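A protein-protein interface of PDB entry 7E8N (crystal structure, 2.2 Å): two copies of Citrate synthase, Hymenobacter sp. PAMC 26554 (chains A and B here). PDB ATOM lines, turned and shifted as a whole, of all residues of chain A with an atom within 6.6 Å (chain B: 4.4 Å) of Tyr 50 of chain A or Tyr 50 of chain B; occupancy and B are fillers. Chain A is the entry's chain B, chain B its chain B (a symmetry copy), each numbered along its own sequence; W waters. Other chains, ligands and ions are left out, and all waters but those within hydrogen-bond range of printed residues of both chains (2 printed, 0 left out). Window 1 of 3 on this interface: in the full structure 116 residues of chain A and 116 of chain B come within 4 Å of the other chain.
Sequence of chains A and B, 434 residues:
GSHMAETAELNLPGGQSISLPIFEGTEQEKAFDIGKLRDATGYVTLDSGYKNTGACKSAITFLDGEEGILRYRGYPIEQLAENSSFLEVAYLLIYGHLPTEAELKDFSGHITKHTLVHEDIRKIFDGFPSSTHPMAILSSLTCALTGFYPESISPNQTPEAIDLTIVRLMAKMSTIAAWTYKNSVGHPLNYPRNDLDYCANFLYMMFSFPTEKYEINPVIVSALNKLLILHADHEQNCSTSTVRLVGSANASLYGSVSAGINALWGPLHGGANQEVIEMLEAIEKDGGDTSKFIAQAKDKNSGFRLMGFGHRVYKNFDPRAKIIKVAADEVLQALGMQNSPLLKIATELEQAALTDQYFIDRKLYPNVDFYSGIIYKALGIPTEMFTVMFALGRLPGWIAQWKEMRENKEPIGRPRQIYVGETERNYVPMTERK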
ATOM      1  N   ASP A  47     -25.990   0.975  -4.264  1.00  0.00           N
ATOM      2  CA  ASP A  47     -26.341  -0.275  -3.543  1.00  0.00           C
ATOM      3  C   ASP A  47     -27.860  -0.475  -3.619  1.00  0.00           C
ATOM      4  O   ASP A  47     -28.604   0.100  -2.789  1.00  0.00           O
ATOM      5  CB  ASP A  47     -25.783  -0.221  -2.116  1.00  0.00           C
ATOM      6  CG  ASP A  47     -25.948  -1.537  -1.394  1.00  0.00           C
ATOM      7  OD1 ASP A  47     -26.075  -2.529  -2.106  1.00  0.00           O
ATOM      8  OD2 ASP A  47     -25.958  -1.546  -0.127  1.00  0.00           O
ATOM      9  N   SER A  48     -28.290  -1.268  -4.592  1.00  0.00           N
ATOM     10  CA  SER A  48     -29.704  -1.651  -4.828  1.00  0.00           C
ATOM     11  C   SER A  48     -30.297  -2.253  -3.547  1.00  0.00           C
ATOM     12  O   SER A  48     -29.886  -3.383  -3.155  1.00  0.00           O
ATOM     13  CB  SER A  48     -29.795  -2.608  -5.991  1.00  0.00           C
ATOM     14  OG  SER A  48     -31.138  -3.015  -6.172  1.00  0.00           O
ATOM     15  N   GLY A  49     -31.218  -1.526  -2.917  1.00  0.00           N
ATOM     16  CA  GLY A  49     -31.991  -2.029  -1.772  1.00  0.00           C
ATOM     17  C   GLY A  49     -31.125  -2.159  -0.530  1.00  0.00           C
ATOM     18  O   GLY A  49     -31.462  -2.981   0.338  1.00  0.00           O
ATOM     19  N   TYR A  50     -30.047  -1.374  -0.455  1.00  0.00           N
ATOM     20  CA  TYR A  50     -29.153  -1.217   0.725  1.00  0.00           C
ATOM     21  C   TYR A  50     -28.594  -2.568   1.171  1.00  0.00           C
ATOM     22  O   TYR A  50     -28.039  -2.623   2.291  1.00  0.00           O
ATOM     23  CB  TYR A  50     -29.870  -0.561   1.900  1.00  0.00           C
ATOM     24  CG  TYR A  50     -30.397   0.830   1.674  1.00  0.00           C
ATOM     25  CD1 TYR A  50     -29.564   1.933   1.603  1.00  0.00           C
ATOM     26  CD2 TYR A  50     -31.754   1.063   1.601  1.00  0.00           C
ATOM     27  CE1 TYR A  50     -30.066   3.221   1.450  1.00  0.00           C
ATOM     28  CE2 TYR A  50     -32.268   2.332   1.416  1.00  0.00           C
ATOM     29  CZ  TYR A  50     -31.426   3.423   1.335  1.00  0.00           C
ATOM     30  OH  TYR A  50     -31.973   4.677   1.216  1.00  0.00           O
ATOM     31  N   LYS A  51     -28.642  -3.555   0.275  1.00  0.00           N
ATOM     32  CA  LYS A  51     -28.269  -4.982   0.468  1.00  0.00           C
ATOM     33  C   LYS A  51     -26.812  -5.147   0.940  1.00  0.00           C
ATOM     34  O   LYS A  51     -26.507  -6.221   1.473  1.00  0.00           O
ATOM     35  CB  LYS A  51     -28.473  -5.710  -0.866  1.00  0.00           C
ATOM     36  CG  LYS A  51     -27.795  -7.071  -1.018  1.00  0.00           C
ATOM     37  CD  LYS A  51     -28.333  -8.137  -0.055  1.00  0.00           C
ATOM     38  CE  LYS A  51     -27.262  -8.909   0.701  1.00  0.00           C
ATOM     39  NZ  LYS A  51     -27.527  -8.911   2.163  1.00  0.00           N
ATOM     40  N   ASN A  52     -25.922  -4.176   0.701  1.00  0.00           N
ATOM     41  CA  ASN A  52     -24.470  -4.295   1.006  1.00  0.00           C
ATOM     42  C   ASN A  52     -24.036  -3.171   1.944  1.00  0.00           C
ATOM     43  O   ASN A  52     -22.831  -2.954   2.082  1.00  0.00           O
ATOM     44  CB  ASN A  52     -23.640  -4.306  -0.262  1.00  0.00           C
ATOM     45  CG  ASN A  52     -23.953  -5.539  -1.090  1.00  0.00           C
ATOM     46  OD1 ASN A  52     -23.318  -6.565  -0.919  1.00  0.00           O
ATOM     47  ND2 ASN A  52     -24.913  -5.450  -1.987  1.00  0.00           N
ATOM     48  N   THR A  53     -24.995  -2.520   2.580  1.00  0.00           N
ATOM     49  CA  THR A  53     -24.795  -1.261   3.327  1.00  0.00           C
ATOM     50  C   THR A  53     -25.165  -1.493   4.790  1.00  0.00           C
ATOM     51  O   THR A  53     -26.327  -1.771   5.078  1.00  0.00           O
ATOM     52  CB  THR A  53     -25.612  -0.106   2.747  1.00  0.00           C
ATOM     53  OG1 THR A  53     -25.181   0.198   1.414  1.00  0.00           O
ATOM     54  CG2 THR A  53     -25.493   1.133   3.603  1.00  0.00           C
ATOM     55  N   GLY A  54     -24.189  -1.328   5.665  1.00  0.00           N
ATOM     56  CA  GLY A  54     -24.395  -1.211   7.116  1.00  0.00           C
ATOM     57  C   GLY A  54     -24.984   0.138   7.433  1.00  0.00           C
ATOM     58  O   GLY A  54     -24.275   1.141   7.375  1.00  0.00           O
ATOM     59  N   ALA A  55     -26.254   0.143   7.773  1.00  0.00           N
ATOM     60  CA  ALA A  55     -27.033   1.353   8.098  1.00  0.00           C
ATOM     61  C   ALA A  55     -26.629   1.830   9.502  1.00  0.00           C
ATOM     62  O   ALA A  55     -26.722   3.004   9.768  1.00  0.00           O
ATOM     63  CB  ALA A  55     -28.507   1.000   8.006  1.00  0.00           C
ATOM     64  N   CYS A  56     -26.143   0.937  10.363  1.00  0.00           N
ATOM     65  CA  CYS A  56     -25.818   1.290  11.760  1.00  0.00           C
ATOM     66  C   CYS A  56     -24.983   0.202  12.418  1.00  0.00           C
ATOM     67  O   CYS A  56     -24.899  -0.951  11.895  1.00  0.00           O
ATOM     68  CB  CYS A  56     -27.091   1.504  12.578  1.00  0.00           C
ATOM     69  SG  CYS A  56     -28.204   0.075  12.580  1.00  0.00           S
ATOM     70  N   SER A 241     -35.892  -0.566   9.511  1.00  0.00           N
ATOM     71  CA  SER A 241     -35.054   0.495   8.920  1.00  0.00           C
ATOM     72  C   SER A 241     -35.934   1.723   8.716  1.00  0.00           C
ATOM     73  O   SER A 241     -35.420   2.837   8.913  1.00  0.00           O
ATOM     74  CB  SER A 241     -34.360   0.030   7.674  1.00  0.00           C
ATOM     75  OG  SER A 241     -33.541  -1.090   7.991  1.00  0.00           O
ATOM     76  N   LEU A 245     -35.145   5.330  10.303  1.00  0.00           N
ATOM     77  CA  LEU A 245     -34.997   6.482   9.380  1.00  0.00           C
ATOM     78  C   LEU A 245     -35.921   7.614   9.823  1.00  0.00           C
ATOM     79  O   LEU A 245     -35.482   8.760   9.953  1.00  0.00           O
ATOM     80  CB  LEU A 245     -35.325   6.033   7.949  1.00  0.00           C
ATOM     81  CG  LEU A 245     -35.142   7.085   6.854  1.00  0.00           C
ATOM     82  CD1 LEU A 245     -33.729   7.659   6.870  1.00  0.00           C
ATOM     83  CD2 LEU A 245     -35.458   6.455   5.476  1.00  0.00           C
ATOM     84  N   ARG A 312     -33.685 -12.820   2.666  1.00  0.00           N
ATOM     85  CA  ARG A 312     -32.664 -11.851   2.201  1.00  0.00           C
ATOM     86  C   ARG A 312     -31.387 -11.973   3.041  1.00  0.00           C
ATOM     87  O   ARG A 312     -30.326 -11.589   2.518  1.00  0.00           O
ATOM     88  CB  ARG A 312     -33.211 -10.428   2.238  1.00  0.00           C
ATOM     89  CG  ARG A 312     -32.311  -9.473   1.480  1.00  0.00           C
ATOM     90  CD  ARG A 312     -32.999  -8.771   0.337  1.00  0.00           C
ATOM     91  NE  ARG A 312     -32.314  -7.507   0.174  1.00  0.00           N
ATOM     92  CZ  ARG A 312     -32.713  -6.535  -0.618  1.00  0.00           C
ATOM     93  NH1 ARG A 312     -33.802  -6.681  -1.358  1.00  0.00           N
ATOM     94  NH2 ARG A 312     -32.009  -5.420  -0.667  1.00  0.00           N
ATOM     95  N   ILE A 412     -29.710  12.747  11.129  1.00  0.00           N
ATOM     96  CA  ILE A 412     -30.916  12.424  10.310  1.00  0.00           C
ATOM     97  C   ILE A 412     -30.430  11.634   9.100  1.00  0.00           C
ATOM     98  O   ILE A 412     -29.425  12.025   8.504  1.00  0.00           O
ATOM     99  CB  ILE A 412     -31.731  13.687   9.942  1.00  0.00           C
ATOM    100  CG1 ILE A 412     -32.970  13.338   9.096  1.00  0.00           C
ATOM    101  CG2 ILE A 412     -30.869  14.755   9.252  1.00  0.00           C
ATOM    102  CD1 ILE A 412     -33.962  14.488   8.960  1.00  0.00           C
ATOM    103  N   GLY A 413     -31.062  10.517   8.773  1.00  0.00           N
ATOM    104  CA  GLY A 413     -30.747   9.785   7.527  1.00  0.00           C
ATOM    105  C   GLY A 413     -30.917  10.703   6.316  1.00  0.00           C
ATOM    106  O   GLY A 413     -31.947  11.344   6.230  1.00  0.00           O
ATOM    107  N   ARG A 414     -29.933  10.798   5.420  1.00  0.00           N
ATOM    108  CA  ARG A 414     -30.034  11.599   4.167  1.00  0.00           C
ATOM    109  C   ARG A 414     -29.272  10.894   3.063  1.00  0.00           C
ATOM    110  O   ARG A 414     -28.135  11.230   2.761  1.00  0.00           O
ATOM    111  CB  ARG A 414     -29.495  13.014   4.406  1.00  0.00           C
ATOM    112  CG  ARG A 414     -30.160  14.070   3.536  1.00  0.00           C
ATOM    113  CD  ARG A 414     -29.708  14.044   2.076  1.00  0.00           C
ATOM    114  NE  ARG A 414     -30.570  14.960   1.342  1.00  0.00           N
ATOM    115  CZ  ARG A 414     -30.796  14.957   0.023  1.00  0.00           C
ATOM    116  NH1 ARG A 414     -30.192  14.088  -0.788  1.00  0.00           N
ATOM    117  NH2 ARG A 414     -31.608  15.885  -0.468  1.00  0.00           N
ATOM    118  N   PRO A 415     -29.838   9.844   2.446  1.00  0.00           N
ATOM    119  CA  PRO A 415     -29.119   9.143   1.387  1.00  0.00           C
ATOM    120  C   PRO A 415     -28.824  10.065   0.209  1.00  0.00           C
ATOM    121  O   PRO A 415     -29.403  11.131   0.158  1.00  0.00           O
ATOM    122  CB  PRO A 415     -30.061   8.023   0.948  1.00  0.00           C
ATOM    123  CG  PRO A 415     -31.081   7.904   2.071  1.00  0.00           C
ATOM    124  CD  PRO A 415     -31.137   9.242   2.765  1.00  0.00           C
ATOM    125  N   ARG A 416     -27.943   9.627  -0.688  1.00  0.00           N
ATOM    126  CA  ARG A 416     -27.649  10.326  -1.959  1.00  0.00           C
ATOM    127  C   ARG A 416     -28.292   9.514  -3.086  1.00  0.00           C
ATOM    128  O   ARG A 416     -28.992   8.532  -2.792  1.00  0.00           O
ATOM    129  CB  ARG A 416     -26.139  10.547  -2.132  1.00  0.00           C
ATOM    130  CG  ARG A 416     -25.460  11.296  -0.977  1.00  0.00           C
ATOM    131  CD  ARG A 416     -25.964  12.704  -0.712  1.00  0.00           C
ATOM    132  NE  ARG A 416     -26.019  13.545  -1.906  1.00  0.00           N
ATOM    133  CZ  ARG A 416     -25.210  14.580  -2.198  1.00  0.00           C
ATOM    134  NH1 ARG A 416     -25.385  15.248  -3.330  1.00  0.00           N
ATOM    135  NH2 ARG A 416     -24.221  14.938  -1.395  1.00  0.00           N
ATOM    136  N   ASP B  47     -21.968   3.459   7.030  1.00  0.00           N
ATOM    137  CA  ASP B  47     -22.244   4.821   6.508  1.00  0.00           C
ATOM    138  C   ASP B  47     -23.302   5.484   7.399  1.00  0.00           C
ATOM    139  O   ASP B  47     -24.518   5.261   7.190  1.00  0.00           O
ATOM    140  CB  ASP B  47     -22.632   4.736   5.026  1.00  0.00           C
ATOM    141  CG  ASP B  47     -22.744   6.102   4.394  1.00  0.00           C
ATOM    142  OD1 ASP B  47     -22.129   7.007   4.950  1.00  0.00           O
ATOM    143  OD2 ASP B  47     -23.457   6.241   3.355  1.00  0.00           O
ATOM    144  N   SER B  48     -22.836   6.270   8.361  1.00  0.00           N
ATOM    145  CA  SER B  48     -23.665   7.056   9.307  1.00  0.00           C
ATOM    146  C   SER B  48     -24.644   7.941   8.525  1.00  0.00           C
ATOM    147  O   SER B  48     -24.191   8.916   7.858  1.00  0.00           O
ATOM    148  CB  SER B  48     -22.780   7.871  10.220  1.00  0.00           C
ATOM    149  OG  SER B  48     -23.580   8.662  11.079  1.00  0.00           O
ATOM    150  N   GLY B  49     -25.933   7.611   8.594  1.00  0.00           N
ATOM    151  CA  GLY B  49     -27.006   8.445   8.033  1.00  0.00           C
ATOM    152  C   GLY B  49     -26.995   8.417   6.514  1.00  0.00           C
ATOM    153  O   GLY B  49     -27.479   9.386   5.905  1.00  0.00           O
ATOM    154  N   TYR B  50     -26.460   7.343   5.928  1.00  0.00           N
ATOM    155  CA  TYR B  50     -26.486   7.030   4.473  1.00  0.00           C
ATOM    156  C   TYR B  50     -25.877   8.172   3.659  1.00  0.00           C
ATOM    157  O   TYR B  50     -26.062   8.159   2.420  1.00  0.00           O
ATOM    158  CB  TYR B  50     -27.900   6.757   3.973  1.00  0.00           C
ATOM    159  CG  TYR B  50     -28.618   5.589   4.593  1.00  0.00           C
ATOM    160  CD1 TYR B  50     -28.290   4.277   4.297  1.00  0.00           C
ATOM    161  CD2 TYR B  50     -29.691   5.792   5.435  1.00  0.00           C
ATOM    162  CE1 TYR B  50     -28.997   3.207   4.832  1.00  0.00           C
ATOM    163  CE2 TYR B  50     -30.383   4.740   6.002  1.00  0.00           C
ATOM    164  CZ  TYR B  50     -30.039   3.436   5.707  1.00  0.00           C
ATOM    165  OH  TYR B  50     -30.790   2.415   6.237  1.00  0.00           O
ATOM    166  N   LYS B  51     -25.101   9.027   4.322  1.00  0.00           N
ATOM    167  CA  LYS B  51     -24.470  10.274   3.812  1.00  0.00           C
ATOM    168  C   LYS B  51     -23.566  10.015   2.592  1.00  0.00           C
ATOM    169  O   LYS B  51     -23.289  10.985   1.875  1.00  0.00           O
ATOM    170  CB  LYS B  51     -23.650  10.892   4.951  1.00  0.00           C
ATOM    171  CG  LYS B  51     -22.614  11.944   4.561  1.00  0.00           C
ATOM    172  CD  LYS B  51     -23.226  13.217   3.961  1.00  0.00           C
ATOM    173  CE  LYS B  51     -22.584  13.681   2.664  1.00  0.00           C
ATOM    174  NZ  LYS B  51     -23.604  13.914   1.607  1.00  0.00           N
ATOM    175  N   ASN B  52     -23.058   8.793   2.389  1.00  0.00           N
ATOM    176  CA  ASN B  52     -22.079   8.475   1.314  1.00  0.00           C
ATOM    177  C   ASN B  52     -22.627   7.372   0.413  1.00  0.00           C
ATOM    178  O   ASN B  52     -21.851   6.799  -0.353  1.00  0.00           O
ATOM    179  CB  ASN B  52     -20.730   8.095   1.892  1.00  0.00           C
ATOM    180  CG  ASN B  52     -20.117   9.274   2.625  1.00  0.00           C
ATOM    181  OD1 ASN B  52     -19.400  10.057   2.026  1.00  0.00           O
ATOM    182  ND2 ASN B  52     -20.378   9.404   3.909  1.00  0.00           N
ATOM    183  N   THR B  53     -23.925   7.126   0.490  1.00  0.00           N
ATOM    184  CA  THR B  53     -24.588   5.951  -0.110  1.00  0.00           C
ATOM    185  C   THR B  53     -25.616   6.434  -1.130  1.00  0.00           C
ATOM    186  O   THR B  53     -26.579   7.094  -0.744  1.00  0.00           O
ATOM    187  CB  THR B  53     -25.255   5.062   0.941  1.00  0.00           C
ATOM    188  OG1 THR B  53     -24.277   4.505   1.827  1.00  0.00           O
ATOM    189  CG2 THR B  53     -26.036   3.941   0.293  1.00  0.00           C
ATOM    190  N   ALA B  55     -28.636   5.536  -2.811  1.00  0.00           N
ATOM    191  CA  ALA B  55     -29.799   4.674  -2.522  1.00  0.00           C
ATOM    192  C   ALA B  55     -30.425   4.237  -3.856  1.00  0.00           C
ATOM    193  O   ALA B  55     -31.018   3.186  -3.905  1.00  0.00           O
ATOM    194  CB  ALA B  55     -30.765   5.465  -1.658  1.00  0.00           C
ATOM    195  N   ARG B 414     -33.518  -3.582   2.252  1.00  0.00           N
ATOM    196  CA  ARG B 414     -33.150  -4.432   3.420  1.00  0.00           C
ATOM    197  C   ARG B 414     -31.725  -4.119   3.832  1.00  0.00           C
ATOM    198  O   ARG B 414     -30.791  -4.827   3.478  1.00  0.00           O
ATOM    199  CB  ARG B 414     -33.319  -5.912   3.064  1.00  0.00           C
ATOM    200  CG  ARG B 414     -33.677  -6.785   4.257  1.00  0.00           C
ATOM    201  CD  ARG B 414     -32.507  -7.050   5.204  1.00  0.00           C
ATOM    202  NE  ARG B 414     -33.047  -7.714   6.381  1.00  0.00           N
ATOM    203  CZ  ARG B 414     -32.481  -7.773   7.593  1.00  0.00           C
ATOM    204  NH1 ARG B 414     -31.290  -7.226   7.836  1.00  0.00           N
ATOM    205  NH2 ARG B 414     -33.123  -8.439   8.544  1.00  0.00           N
ATOM    206  N   PRO B 415     -31.481  -3.012   4.550  1.00  0.00           N
ATOM    207  CA  PRO B 415     -30.115  -2.684   4.949  1.00  0.00           C
ATOM    208  C   PRO B 415     -29.523  -3.766   5.846  1.00  0.00           C
ATOM    209  O   PRO B 415     -30.277  -4.593   6.319  1.00  0.00           O
ATOM    210  CB  PRO B 415     -30.237  -1.374   5.724  1.00  0.00           C
ATOM    211  CG  PRO B 415     -31.608  -0.825   5.358  1.00  0.00           C
ATOM    212  CD  PRO B 415     -32.463  -1.999   4.954  1.00  0.00           C
ATOM    213  N   ARG B 416     -28.207  -3.723   6.048  1.00  0.00           N
ATOM    214  CA  ARG B 416     -27.494  -4.603   7.000  1.00  0.00           C
ATOM    215  C   ARG B 416     -27.099  -3.746   8.205  1.00  0.00           C
ATOM    216  O   ARG B 416     -27.487  -2.568   8.256  1.00  0.00           O
ATOM    217  CB  ARG B 416     -26.311  -5.307   6.320  1.00  0.00           C
ATOM    218  CG  ARG B 416     -26.674  -6.113   5.065  1.00  0.00           C
ATOM    219  CD  ARG B 416     -27.654  -7.254   5.271  1.00  0.00           C
ATOM    220  NE  ARG B 416     -27.295  -8.150   6.368  1.00  0.00           N
ATOM    221  CZ  ARG B 416     -26.841  -9.411   6.261  1.00  0.00           C
ATOM    222  NH1 ARG B 416     -26.554 -10.100   7.356  1.00  0.00           N
ATOM    223  NH2 ARG B 416     -26.646  -9.982   5.083  1.00  0.00           N
HETATM  224  O   HOH W   1     -32.575   3.175   8.698  1.00  0.00           O
HETATM  225  O   HOH W   2     -22.999   2.041   1.073  1.00  0.00           O
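N of Ala 55 of chain B is in hydrogen-bond range of O of Arg 416 of chain A, at 3.0 Å.
The backbone carbonyl oxygen (O) of Gly 49 of chain A is in hydrogen-bond range of the backbone NH (N) of Arg 414 of chain B (2.9 Å).
The backbone carbonyl oxygen (O) of Thr 53 of chain A sits at hydrogen-bond distance from the backbone NH (N) of Arg 416 of chain B.
O of Gly 54 of chain A lies within hydrogen-bond range of N of Asp 47 of chain B (3.3 Å).
NZ of Lys 51 of chain B sits close to NH2 of Arg 416 of chain A (3.2 Å).
The backbone carbonyl oxygen (O) of Thr 53 of chain B is in hydrogen-bond range of the backbone NH (N) of Arg 416 of chain A, at 2.9 Å.
NH2 of Arg 416 of chain B sits close to NZ of Lys 51 of chain A (3.2 Å).
O of Arg 416 of chain B lies within hydrogen-bond range of N of Ala 55 of chain A, 3.0 Å away.
O of Gly 49 of chain B sits at hydrogen-bond distance from N of Arg 414 of chain A (2.9 Å).
The backbone NH (N) of Lys 51 of chain A lies within hydrogen-bond range of the side-chain carboxylate (OD2) of Asp 47 of chain A.
The backbone carbonyl oxygen (O) of Gly 49 of chain A sits at hydrogen-bond distance from the guanidinium group (NH2) of Arg 312 of chain A (2.7 Å).
The side-chain carboxylate (OD2) of Asp 47 of chain B sits at hydrogen-bond distance from the backbone NH (N) of Asn 52 of chain B (2.8 Å).
OD2 of Asp 47 of chain B is in hydrogen-bond range of OG1 of Thr 53 of chain B (2.5 Å).
OD2 of Asp 47 of chain B sits at hydrogen-bond distance from N of Lys 51 of chain B (3.4 Å).
The side-chain hydroxyl (OG1) of Thr 53 of chain A sits at hydrogen-bond distance from the side-chain carboxylate (OD2) of Asp 47 of chain A, 2.5 Å away.
Among the printed residues, merely in contact across the chains: Tyr 50 of chain A with Ala 55 of chain B, Ala 55 of chain A with Tyr 50 of chain B, Ser 241 of chain A with Pro 415 of chain B, Tyr 50 of chain A with Pro 415 of chain B, Pro 415 of chain A with Tyr 50 of chain B, Arg 312 of chain A with Arg 414 of chain B, Tyr 50 of chain A with Tyr 50 of chain B, Gly 54 of chain A with Arg 416 of chain B, Gly 413 of chain A with Gly 49 of chain B, Pro 415 of chain A with Ala 55 of chain B, Ala 55 of chain A with Pro 415 of chain B, Tyr 50 of chain A with Arg 414 of chain B, Arg 414 of chain A with Tyr 50 of chain B, Pro 415 of chain A with Thr 53 of chain B, Thr 53 of chain A with Pro 415 of chain B, Arg 416 of chain A with Tyr 50 of chain B, Tyr 50 of chain A with Arg 416 of chain B, Lys 51 of chain A with Arg 414 of chain B, Arg 414 of chain A with Lys 51 of chain B and Thr 53 of chain A with Thr 53 of chain B.
Of chain A, only Tyr 50, Ala 55, Arg 414, Pro 415 and Arg 416 come within 4 Å of Tyr 50 of chain B.
Printed residues of chain A within 4 Å of Pro 415 of chain B: Tyr 50 (3.4 Å), Thr 53 (3.8 Å), Ala 55 (3.7 Å) and Ser 241 (3.3 Å).
Printed residues of chain A within 4 Å of Arg 416 of chain B: Tyr 50, Lys 51, Thr 53, Gly 54 and Ala 55.
The nearest printed residue of chain A that does not touch Arg 414 of chain B is Ser 241 of chain A (5.5 Å).
Of the 11 printed residues of chain B, 9 touch a printed residue of chain A.
Hydrophobic or aromatic side chains of chain B that line the printed part of chain A: Tyr 50, Ala 55 and Pro 415.
Among the printed residues, 29 pairs touch across the chains.
Among the printed residues, no Asp or Glu carboxylate lies within 4 Å of a Lys or Arg side-chain nitrogen of the other chain.
Gly 49 of chain A touches Arg 414 of chain B, and with the chains exchanged Arg 414 of chain A touches Gly 49 of chain B.
Tyr 50 of chain A touches Arg 414 of chain B, and with the chains exchanged Arg 414 of chain A touches Tyr 50 of chain B.
Thr 53 of chain A touches its own counterpart, Thr 53 of chain B.
Thr 53 of chain A touches Arg 416 of chain B, and with the chains exchanged Arg 416 of chain A touches Thr 53 of chain B.
Positions printed for both chains: 47, 48, 49, 50, 51, 52, 53, 55, 414, 415 and 416.
Water W1 bridges O of Ser 241 of chain A and OH of Tyr 50 of chain B.
Water W2 bridges OG1 of Thr 53 of chain B (2.9 Å) and OG1 of Thr 53 of chain A (2.9 Å).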
